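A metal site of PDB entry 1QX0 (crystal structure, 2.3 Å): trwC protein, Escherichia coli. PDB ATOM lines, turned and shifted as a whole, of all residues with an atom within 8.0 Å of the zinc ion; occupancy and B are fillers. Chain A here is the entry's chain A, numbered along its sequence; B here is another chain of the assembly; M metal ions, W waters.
O of His 163 lies within hydrogen-bond range of N of Phe 148 (2.8 Å). NE2 of His 150 lies within hydrogen-bond range of O of Tyr 18 (2.8 Å). A ring nitrogen (ND1) of His 163 sits at hydrogen-bond distance from the side-chain hydroxyl (OG1) of Thr 87 (3.1 Å). The side-chain carboxylate of Asp 85 sits at hydrogen-bond distance from a ring nitrogen (ND1) of His 163, 3.1 Å away. O of Gln 159 is in hydrogen-bond range of ND1 of His 161 (2.8 Å). O of Asp 21 lies close to NE2 of His 150 (3.2 Å).
The nearest printed residue that does not touch the zinc ion is Asp 21 (4.8 Å).
The zinc ion is bound by ND1 of His 150. NE2 of His 161 binds the zinc ion. NE2 of His 163 is bound to the zinc ion. The zinc ion is bound by water W1 (2.5 Å). The zinc ion has four donor atoms within binding distance.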
ATOM      1  N   SER A  17      30.127 -11.474 -23.000  1.00  0.00           N
ATOM      2  CA  SER A  17      29.661 -11.787 -24.358  1.00  0.00           C
ATOM      3  C   SER A  17      29.293 -10.531 -25.159  1.00  0.00           C
ATOM      4  O   SER A  17      28.713 -10.633 -26.245  1.00  0.00           O
ATOM      5  CB  SER A  17      28.469 -12.739 -24.302  1.00  0.00           C
ATOM      6  OG  SER A  17      27.254 -12.024 -24.178  1.00  0.00           O
ATOM      7  N   TYR A  18      29.623  -9.360 -24.640  1.00  0.00           N
ATOM      8  CA  TYR A  18      29.494  -8.111 -25.379  1.00  0.00           C
ATOM      9  C   TYR A  18      30.466  -8.054 -26.567  1.00  0.00           C
ATOM     10  O   TYR A  18      30.525  -7.067 -27.286  1.00  0.00           O
ATOM     11  CB  TYR A  18      29.594  -6.908 -24.444  1.00  0.00           C
ATOM     12  CG  TYR A  18      28.371  -6.714 -23.575  1.00  0.00           C
ATOM     13  CD1 TYR A  18      27.090  -7.128 -24.011  1.00  0.00           C
ATOM     14  CD2 TYR A  18      28.472  -6.130 -22.316  1.00  0.00           C
ATOM     15  CE1 TYR A  18      25.957  -6.958 -23.203  1.00  0.00           C
ATOM     16  CE2 TYR A  18      27.338  -5.944 -21.495  1.00  0.00           C
ATOM     17  CZ  TYR A  18      26.091  -6.358 -21.946  1.00  0.00           C
ATOM     18  OH  TYR A  18      24.979  -6.181 -21.145  1.00  0.00           O
ATOM     19  N   GLU A  20      29.948 -10.719 -28.716  1.00  0.00           N
ATOM     20  CA  GLU A  20      29.192 -11.568 -29.627  1.00  0.00           C
ATOM     21  C   GLU A  20      28.469 -10.847 -30.785  1.00  0.00           C
ATOM     22  O   GLU A  20      28.676 -11.213 -31.950  1.00  0.00           O
ATOM     23  CB  GLU A  20      28.255 -12.505 -28.857  1.00  0.00           C
ATOM     24  CG  GLU A  20      29.012 -13.545 -28.032  1.00  0.00           C
ATOM     25  CD  GLU A  20      28.256 -14.869 -27.927  1.00  0.00           C
ATOM     26  OE1 GLU A  20      28.876 -15.939 -28.163  1.00  0.00           O
ATOM     27  OE2 GLU A  20      27.037 -14.836 -27.608  1.00  0.00           O
ATOM     28  N   ASP A  21      27.632  -9.850 -30.486  1.00  0.00           N
ATOM     29  CA  ASP A  21      27.081  -9.003 -31.571  1.00  0.00           C
ATOM     30  C   ASP A  21      28.159  -8.004 -31.963  1.00  0.00           C
ATOM     31  O   ASP A  21      28.133  -6.839 -31.555  1.00  0.00           O
ATOM     32  CB  ASP A  21      25.775  -8.302 -31.128  1.00  0.00           C
ATOM     33  CG  ASP A  21      25.173  -7.375 -32.231  1.00  0.00           C
ATOM     34  OD1 ASP A  21      24.035  -6.905 -32.019  1.00  0.00           O
ATOM     35  OD2 ASP A  21      25.738  -7.062 -33.300  1.00  0.00           O
ATOM     36  N   GLY A  22      29.125  -8.448 -32.764  1.00  0.00           N
ATOM     37  CA  GLY A  22      30.232  -7.589 -33.129  1.00  0.00           C
ATOM     38  C   GLY A  22      31.204  -8.183 -34.124  1.00  0.00           C
ATOM     39  O   GLY A  22      31.932  -7.459 -34.792  1.00  0.00           O
ATOM     40  N   ASP A  25      29.614  -7.592 -37.453  1.00  0.00           N
ATOM     41  CA  ASP A  25      29.205  -6.182 -37.529  1.00  0.00           C
ATOM     42  C   ASP A  25      29.470  -5.411 -38.836  1.00  0.00           C
ATOM     43  O   ASP A  25      28.609  -4.661 -39.295  1.00  0.00           O
ATOM     44  CB  ASP A  25      29.774  -5.401 -36.330  1.00  0.00           C
ATOM     45  CG  ASP A  25      28.748  -5.219 -35.210  1.00  0.00           C
ATOM     46  OD1 ASP A  25      27.573  -5.595 -35.395  1.00  0.00           O
ATOM     47  OD2 ASP A  25      29.034  -4.698 -34.117  1.00  0.00           O
ATOM     48  N   ASP A  85      27.110  -1.082 -16.431  1.00  0.00           N
ATOM     49  CA  ASP A  85      26.959  -0.993 -17.847  1.00  0.00           C
ATOM     50  C   ASP A  85      26.196   0.290 -18.156  1.00  0.00           C
ATOM     51  O   ASP A  85      25.058   0.480 -17.696  1.00  0.00           O
ATOM     52  CB  ASP A  85      26.220  -2.236 -18.405  1.00  0.00           C
ATOM     53  CG  ASP A  85      26.056  -2.173 -19.945  1.00  0.00           C
ATOM     54  OD1 ASP A  85      26.602  -1.217 -20.566  1.00  0.00           O
ATOM     55  OD2 ASP A  85      25.407  -3.006 -20.625  1.00  0.00           O
ATOM     56  N   THR A  87      24.677   1.992 -21.381  1.00  0.00           N
ATOM     57  CA  THR A  87      24.430   1.593 -22.769  1.00  0.00           C
ATOM     58  C   THR A  87      23.953   2.834 -23.511  1.00  0.00           C
ATOM     59  O   THR A  87      22.902   3.368 -23.201  1.00  0.00           O
ATOM     60  CB  THR A  87      23.408   0.411 -22.822  1.00  0.00           C
ATOM     61  OG1 THR A  87      23.977  -0.766 -22.198  1.00  0.00           O
ATOM     62  CG2 THR A  87      23.101  -0.011 -24.277  1.00  0.00           C
ATOM     63  N   SER A  89      22.559   4.648 -26.845  1.00  0.00           N
ATOM     64  CA  SER A  89      21.838   4.254 -28.085  1.00  0.00           C
ATOM     65  C   SER A  89      21.510   5.444 -28.902  1.00  0.00           C
ATOM     66  O   SER A  89      20.927   6.388 -28.395  1.00  0.00           O
ATOM     67  CB  SER A  89      20.533   3.527 -27.728  1.00  0.00           C
ATOM     68  OG  SER A  89      20.859   2.330 -27.057  1.00  0.00           O
ATOM     69  N   PHE A 148      31.914  -1.619 -25.896  1.00  0.00           N
ATOM     70  CA  PHE A 148      31.536  -2.585 -26.934  1.00  0.00           C
ATOM     71  C   PHE A 148      30.440  -2.015 -27.821  1.00  0.00           C
ATOM     72  O   PHE A 148      29.271  -1.916 -27.424  1.00  0.00           O
ATOM     73  CB  PHE A 148      31.125  -3.927 -26.288  1.00  0.00           C
ATOM     74  CG  PHE A 148      32.145  -4.464 -25.334  1.00  0.00           C
ATOM     75  CD1 PHE A 148      32.110  -4.126 -23.976  1.00  0.00           C
ATOM     76  CD2 PHE A 148      33.202  -5.274 -25.797  1.00  0.00           C
ATOM     77  CE1 PHE A 148      33.086  -4.616 -23.079  1.00  0.00           C
ATOM     78  CE2 PHE A 148      34.175  -5.746 -24.921  1.00  0.00           C
ATOM     79  CZ  PHE A 148      34.118  -5.391 -23.554  1.00  0.00           C
ATOM     80  N   ARG A 149      30.831  -1.597 -29.018  1.00  0.00           N
ATOM     81  CA  ARG A 149      29.893  -1.021 -29.969  1.00  0.00           C
ATOM     82  C   ARG A 149      29.188  -2.119 -30.772  1.00  0.00           C
ATOM     83  O   ARG A 149      29.828  -3.059 -31.266  1.00  0.00           O
ATOM     84  CB  ARG A 149      30.600  -0.030 -30.902  1.00  0.00           C
ATOM     85  CG  ARG A 149      29.638   0.848 -31.714  1.00  0.00           C
ATOM     86  CD  ARG A 149      30.255   1.663 -32.829  1.00  0.00           C
ATOM     87  NE  ARG A 149      30.903   0.821 -33.792  1.00  0.00           N
ATOM     88  CZ  ARG A 149      32.174   0.940 -34.195  1.00  0.00           C
ATOM     89  NH1 ARG A 149      32.637   0.079 -35.081  1.00  0.00           N
ATOM     90  NH2 ARG A 149      32.950   1.921 -33.745  1.00  0.00           N
ATOM     91  N   HIS A 150      27.864  -1.982 -30.901  1.00  0.00           N
ATOM     92  CA  HIS A 150      27.011  -2.971 -31.543  1.00  0.00           C
ATOM     93  C   HIS A 150      26.129  -2.268 -32.563  1.00  0.00           C
ATOM     94  O   HIS A 150      25.949  -1.069 -32.478  1.00  0.00           O
ATOM     95  CB  HIS A 150      26.141  -3.625 -30.487  1.00  0.00           C
ATOM     96  CG  HIS A 150      26.886  -4.532 -29.556  1.00  0.00           C
ATOM     97  ND1 HIS A 150      26.284  -5.164 -28.500  1.00  0.00           N
ATOM     98  CD2 HIS A 150      28.175  -4.944 -29.554  1.00  0.00           C
ATOM     99  CE1 HIS A 150      27.165  -5.924 -27.875  1.00  0.00           C
ATOM    100  NE2 HIS A 150      28.327  -5.805 -28.496  1.00  0.00           N
ATOM    101  N   GLU A 151      25.547  -3.034 -33.504  1.00  0.00           N
ATOM    102  CA  GLU A 151      24.845  -2.434 -34.628  1.00  0.00           C
ATOM    103  C   GLU A 151      23.413  -2.899 -34.842  1.00  0.00           C
ATOM    104  O   GLU A 151      22.734  -2.370 -35.713  1.00  0.00           O
ATOM    105  CB  GLU A 151      25.652  -2.629 -35.941  1.00  0.00           C
ATOM    106  CG  GLU A 151      27.077  -2.113 -35.879  1.00  0.00           C
ATOM    107  CD  GLU A 151      27.891  -2.352 -37.156  1.00  0.00           C
ATOM    108  OE1 GLU A 151      27.376  -3.049 -38.067  1.00  0.00           O
ATOM    109  OE2 GLU A 151      29.034  -1.830 -37.235  1.00  0.00           O
ATOM    110  N   THR A 152      22.943  -3.875 -34.072  1.00  0.00           N
ATOM    111  CA  THR A 152      21.616  -4.450 -34.338  1.00  0.00           C
ATOM    112  C   THR A 152      20.776  -4.666 -33.100  1.00  0.00           C
ATOM    113  O   THR A 152      21.317  -4.914 -32.007  1.00  0.00           O
ATOM    114  CB  THR A 152      21.694  -5.791 -35.137  1.00  0.00           C
ATOM    115  OG1 THR A 152      22.196  -6.829 -34.292  1.00  0.00           O
ATOM    116  CG2 THR A 152      22.723  -5.748 -36.243  1.00  0.00           C
ATOM    117  N   SER A 153      19.447  -4.594 -33.291  1.00  0.00           N
ATOM    118  CA  SER A 153      18.508  -4.779 -32.199  1.00  0.00           C
ATOM    119  C   SER A 153      18.209  -6.257 -32.068  1.00  0.00           C
ATOM    120  O   SER A 153      18.582  -7.060 -32.948  1.00  0.00           O
ATOM    121  CB  SER A 153      17.219  -3.952 -32.379  1.00  0.00           C
ATOM    122  OG  SER A 153      16.262  -4.584 -33.227  1.00  0.00           O
ATOM    123  N   ARG A 154      17.549  -6.620 -30.990  1.00  0.00           N
ATOM    124  CA  ARG A 154      17.109  -8.017 -30.835  1.00  0.00           C
ATOM    125  C   ARG A 154      16.154  -8.424 -31.977  1.00  0.00           C
ATOM    126  O   ARG A 154      16.054  -9.598 -32.270  1.00  0.00           O
ATOM    127  CB  ARG A 154      16.561  -8.269 -29.437  1.00  0.00           C
ATOM    128  CG  ARG A 154      17.637  -8.001 -28.376  1.00  0.00           C
ATOM    129  CD  ARG A 154      17.256  -8.305 -26.896  1.00  0.00           C
ATOM    130  NE  ARG A 154      17.216  -9.757 -26.585  1.00  0.00           N
ATOM    131  CZ  ARG A 154      18.116 -10.414 -25.865  1.00  0.00           C
ATOM    132  NH1 ARG A 154      19.177  -9.782 -25.352  1.00  0.00           N
ATOM    133  NH2 ARG A 154      17.970 -11.717 -25.655  1.00  0.00           N
ATOM    134  N   GLN A 159      20.519  -0.587 -35.195  1.00  0.00           N
ATOM    135  CA  GLN A 159      20.400  -0.094 -33.822  1.00  0.00           C
ATOM    136  C   GLN A 159      21.800   0.198 -33.284  1.00  0.00           C
ATOM    137  O   GLN A 159      22.412  -0.663 -32.659  1.00  0.00           O
ATOM    138  CB  GLN A 159      19.681  -1.139 -32.934  1.00  0.00           C
ATOM    139  CG  GLN A 159      19.441  -0.726 -31.472  1.00  0.00           C
ATOM    140  CD  GLN A 159      18.678   0.610 -31.305  1.00  0.00           C
ATOM    141  OE1 GLN A 159      18.105   1.179 -32.251  1.00  0.00           O
ATOM    142  NE2 GLN A 159      18.678   1.103 -30.081  1.00  0.00           N
ATOM    143  N   LEU A 160      22.332   1.380 -33.617  1.00  0.00           N
ATOM    144  CA  LEU A 160      23.696   1.712 -33.235  1.00  0.00           C
ATOM    145  C   LEU A 160      23.676   1.981 -31.750  1.00  0.00           C
ATOM    146  O   LEU A 160      23.055   2.945 -31.267  1.00  0.00           O
ATOM    147  CB  LEU A 160      24.213   2.949 -34.015  1.00  0.00           C
ATOM    148  CG  LEU A 160      25.652   3.497 -33.806  1.00  0.00           C
ATOM    149  CD1 LEU A 160      26.722   2.460 -34.081  1.00  0.00           C
ATOM    150  CD2 LEU A 160      25.871   4.656 -34.767  1.00  0.00           C
ATOM    151  N   HIS A 161      24.354   1.123 -31.002  1.00  0.00           N
ATOM    152  CA  HIS A 161      24.503   1.315 -29.560  1.00  0.00           C
ATOM    153  C   HIS A 161      25.840   0.848 -29.061  1.00  0.00           C
ATOM    154  O   HIS A 161      26.440  -0.053 -29.665  1.00  0.00           O
ATOM    155  CB  HIS A 161      23.367   0.613 -28.795  1.00  0.00           C
ATOM    156  CG  HIS A 161      23.347  -0.871 -28.954  1.00  0.00           C
ATOM    157  ND1 HIS A 161      22.765  -1.504 -30.034  1.00  0.00           N
ATOM    158  CD2 HIS A 161      23.799  -1.855 -28.129  1.00  0.00           C
ATOM    159  CE1 HIS A 161      22.851  -2.813 -29.872  1.00  0.00           C
ATOM    160  NE2 HIS A 161      23.480  -3.050 -28.727  1.00  0.00           N
ATOM    161  N   THR A 162      26.295   1.412 -27.937  1.00  0.00           N
ATOM    162  CA  THR A 162      27.551   1.000 -27.304  1.00  0.00           C
ATOM    163  C   THR A 162      27.338   0.656 -25.818  1.00  0.00           C
ATOM    164  O   THR A 162      26.758   1.431 -25.082  1.00  0.00           O
ATOM    165  CB  THR A 162      28.610   2.141 -27.385  1.00  0.00           C
ATOM    166  OG1 THR A 162      28.989   2.401 -28.752  1.00  0.00           O
ATOM    167  CG2 THR A 162      29.892   1.721 -26.697  1.00  0.00           C
ATOM    168  N   HIS A 163      27.861  -0.488 -25.402  1.00  0.00           N
ATOM    169  CA  HIS A 163      27.832  -0.883 -24.005  1.00  0.00           C
ATOM    170  C   HIS A 163      29.142  -0.434 -23.422  1.00  0.00           C
ATOM    171  O   HIS A 163      30.198  -0.976 -23.768  1.00  0.00           O
ATOM    172  CB  HIS A 163      27.729  -2.392 -23.845  1.00  0.00           C
ATOM    173  CG  HIS A 163      26.489  -2.975 -24.422  1.00  0.00           C
ATOM    174  ND1 HIS A 163      25.307  -3.058 -23.720  1.00  0.00           N
ATOM    175  CD2 HIS A 163      26.258  -3.564 -25.618  1.00  0.00           C
ATOM    176  CE1 HIS A 163      24.397  -3.662 -24.475  1.00  0.00           C
ATOM    177  NE2 HIS A 163      24.948  -3.971 -25.633  1.00  0.00           N
ATOM    178  P    DT B  25      15.921  -4.566 -26.832  1.00  0.00           P
ATOM    179  OP1  DT B  25      16.628  -4.753 -28.143  1.00  0.00           O
ATOM    180  OP2  DT B  25      14.703  -5.371 -26.657  1.00  0.00           O
ATOM    181  O5'  DT B  25      16.834  -4.657 -25.511  1.00  0.00           O
ATOM    182  C5'  DT B  25      18.255  -4.853 -25.587  1.00  0.00           C
ATOM    183  C4'  DT B  25      18.891  -4.612 -24.232  1.00  0.00           C
ATOM    184  O4'  DT B  25      18.743  -5.805 -23.413  1.00  0.00           O
ATOM    185  C3'  DT B  25      20.397  -4.413 -24.228  1.00  0.00           C
ATOM    186  O3'  DT B  25      20.781  -3.129 -24.714  1.00  0.00           O
ATOM    187  C2'  DT B  25      20.686  -4.650 -22.743  1.00  0.00           C
ATOM    188  C1'  DT B  25      19.812  -5.887 -22.481  1.00  0.00           C
HETATM  189 ZN    ZN M   1      24.412  -4.715 -27.721  1.00  0.00          ZN
HETATM  190  O   HOH W   1      22.114  -5.300 -26.947  1.00  0.00           O
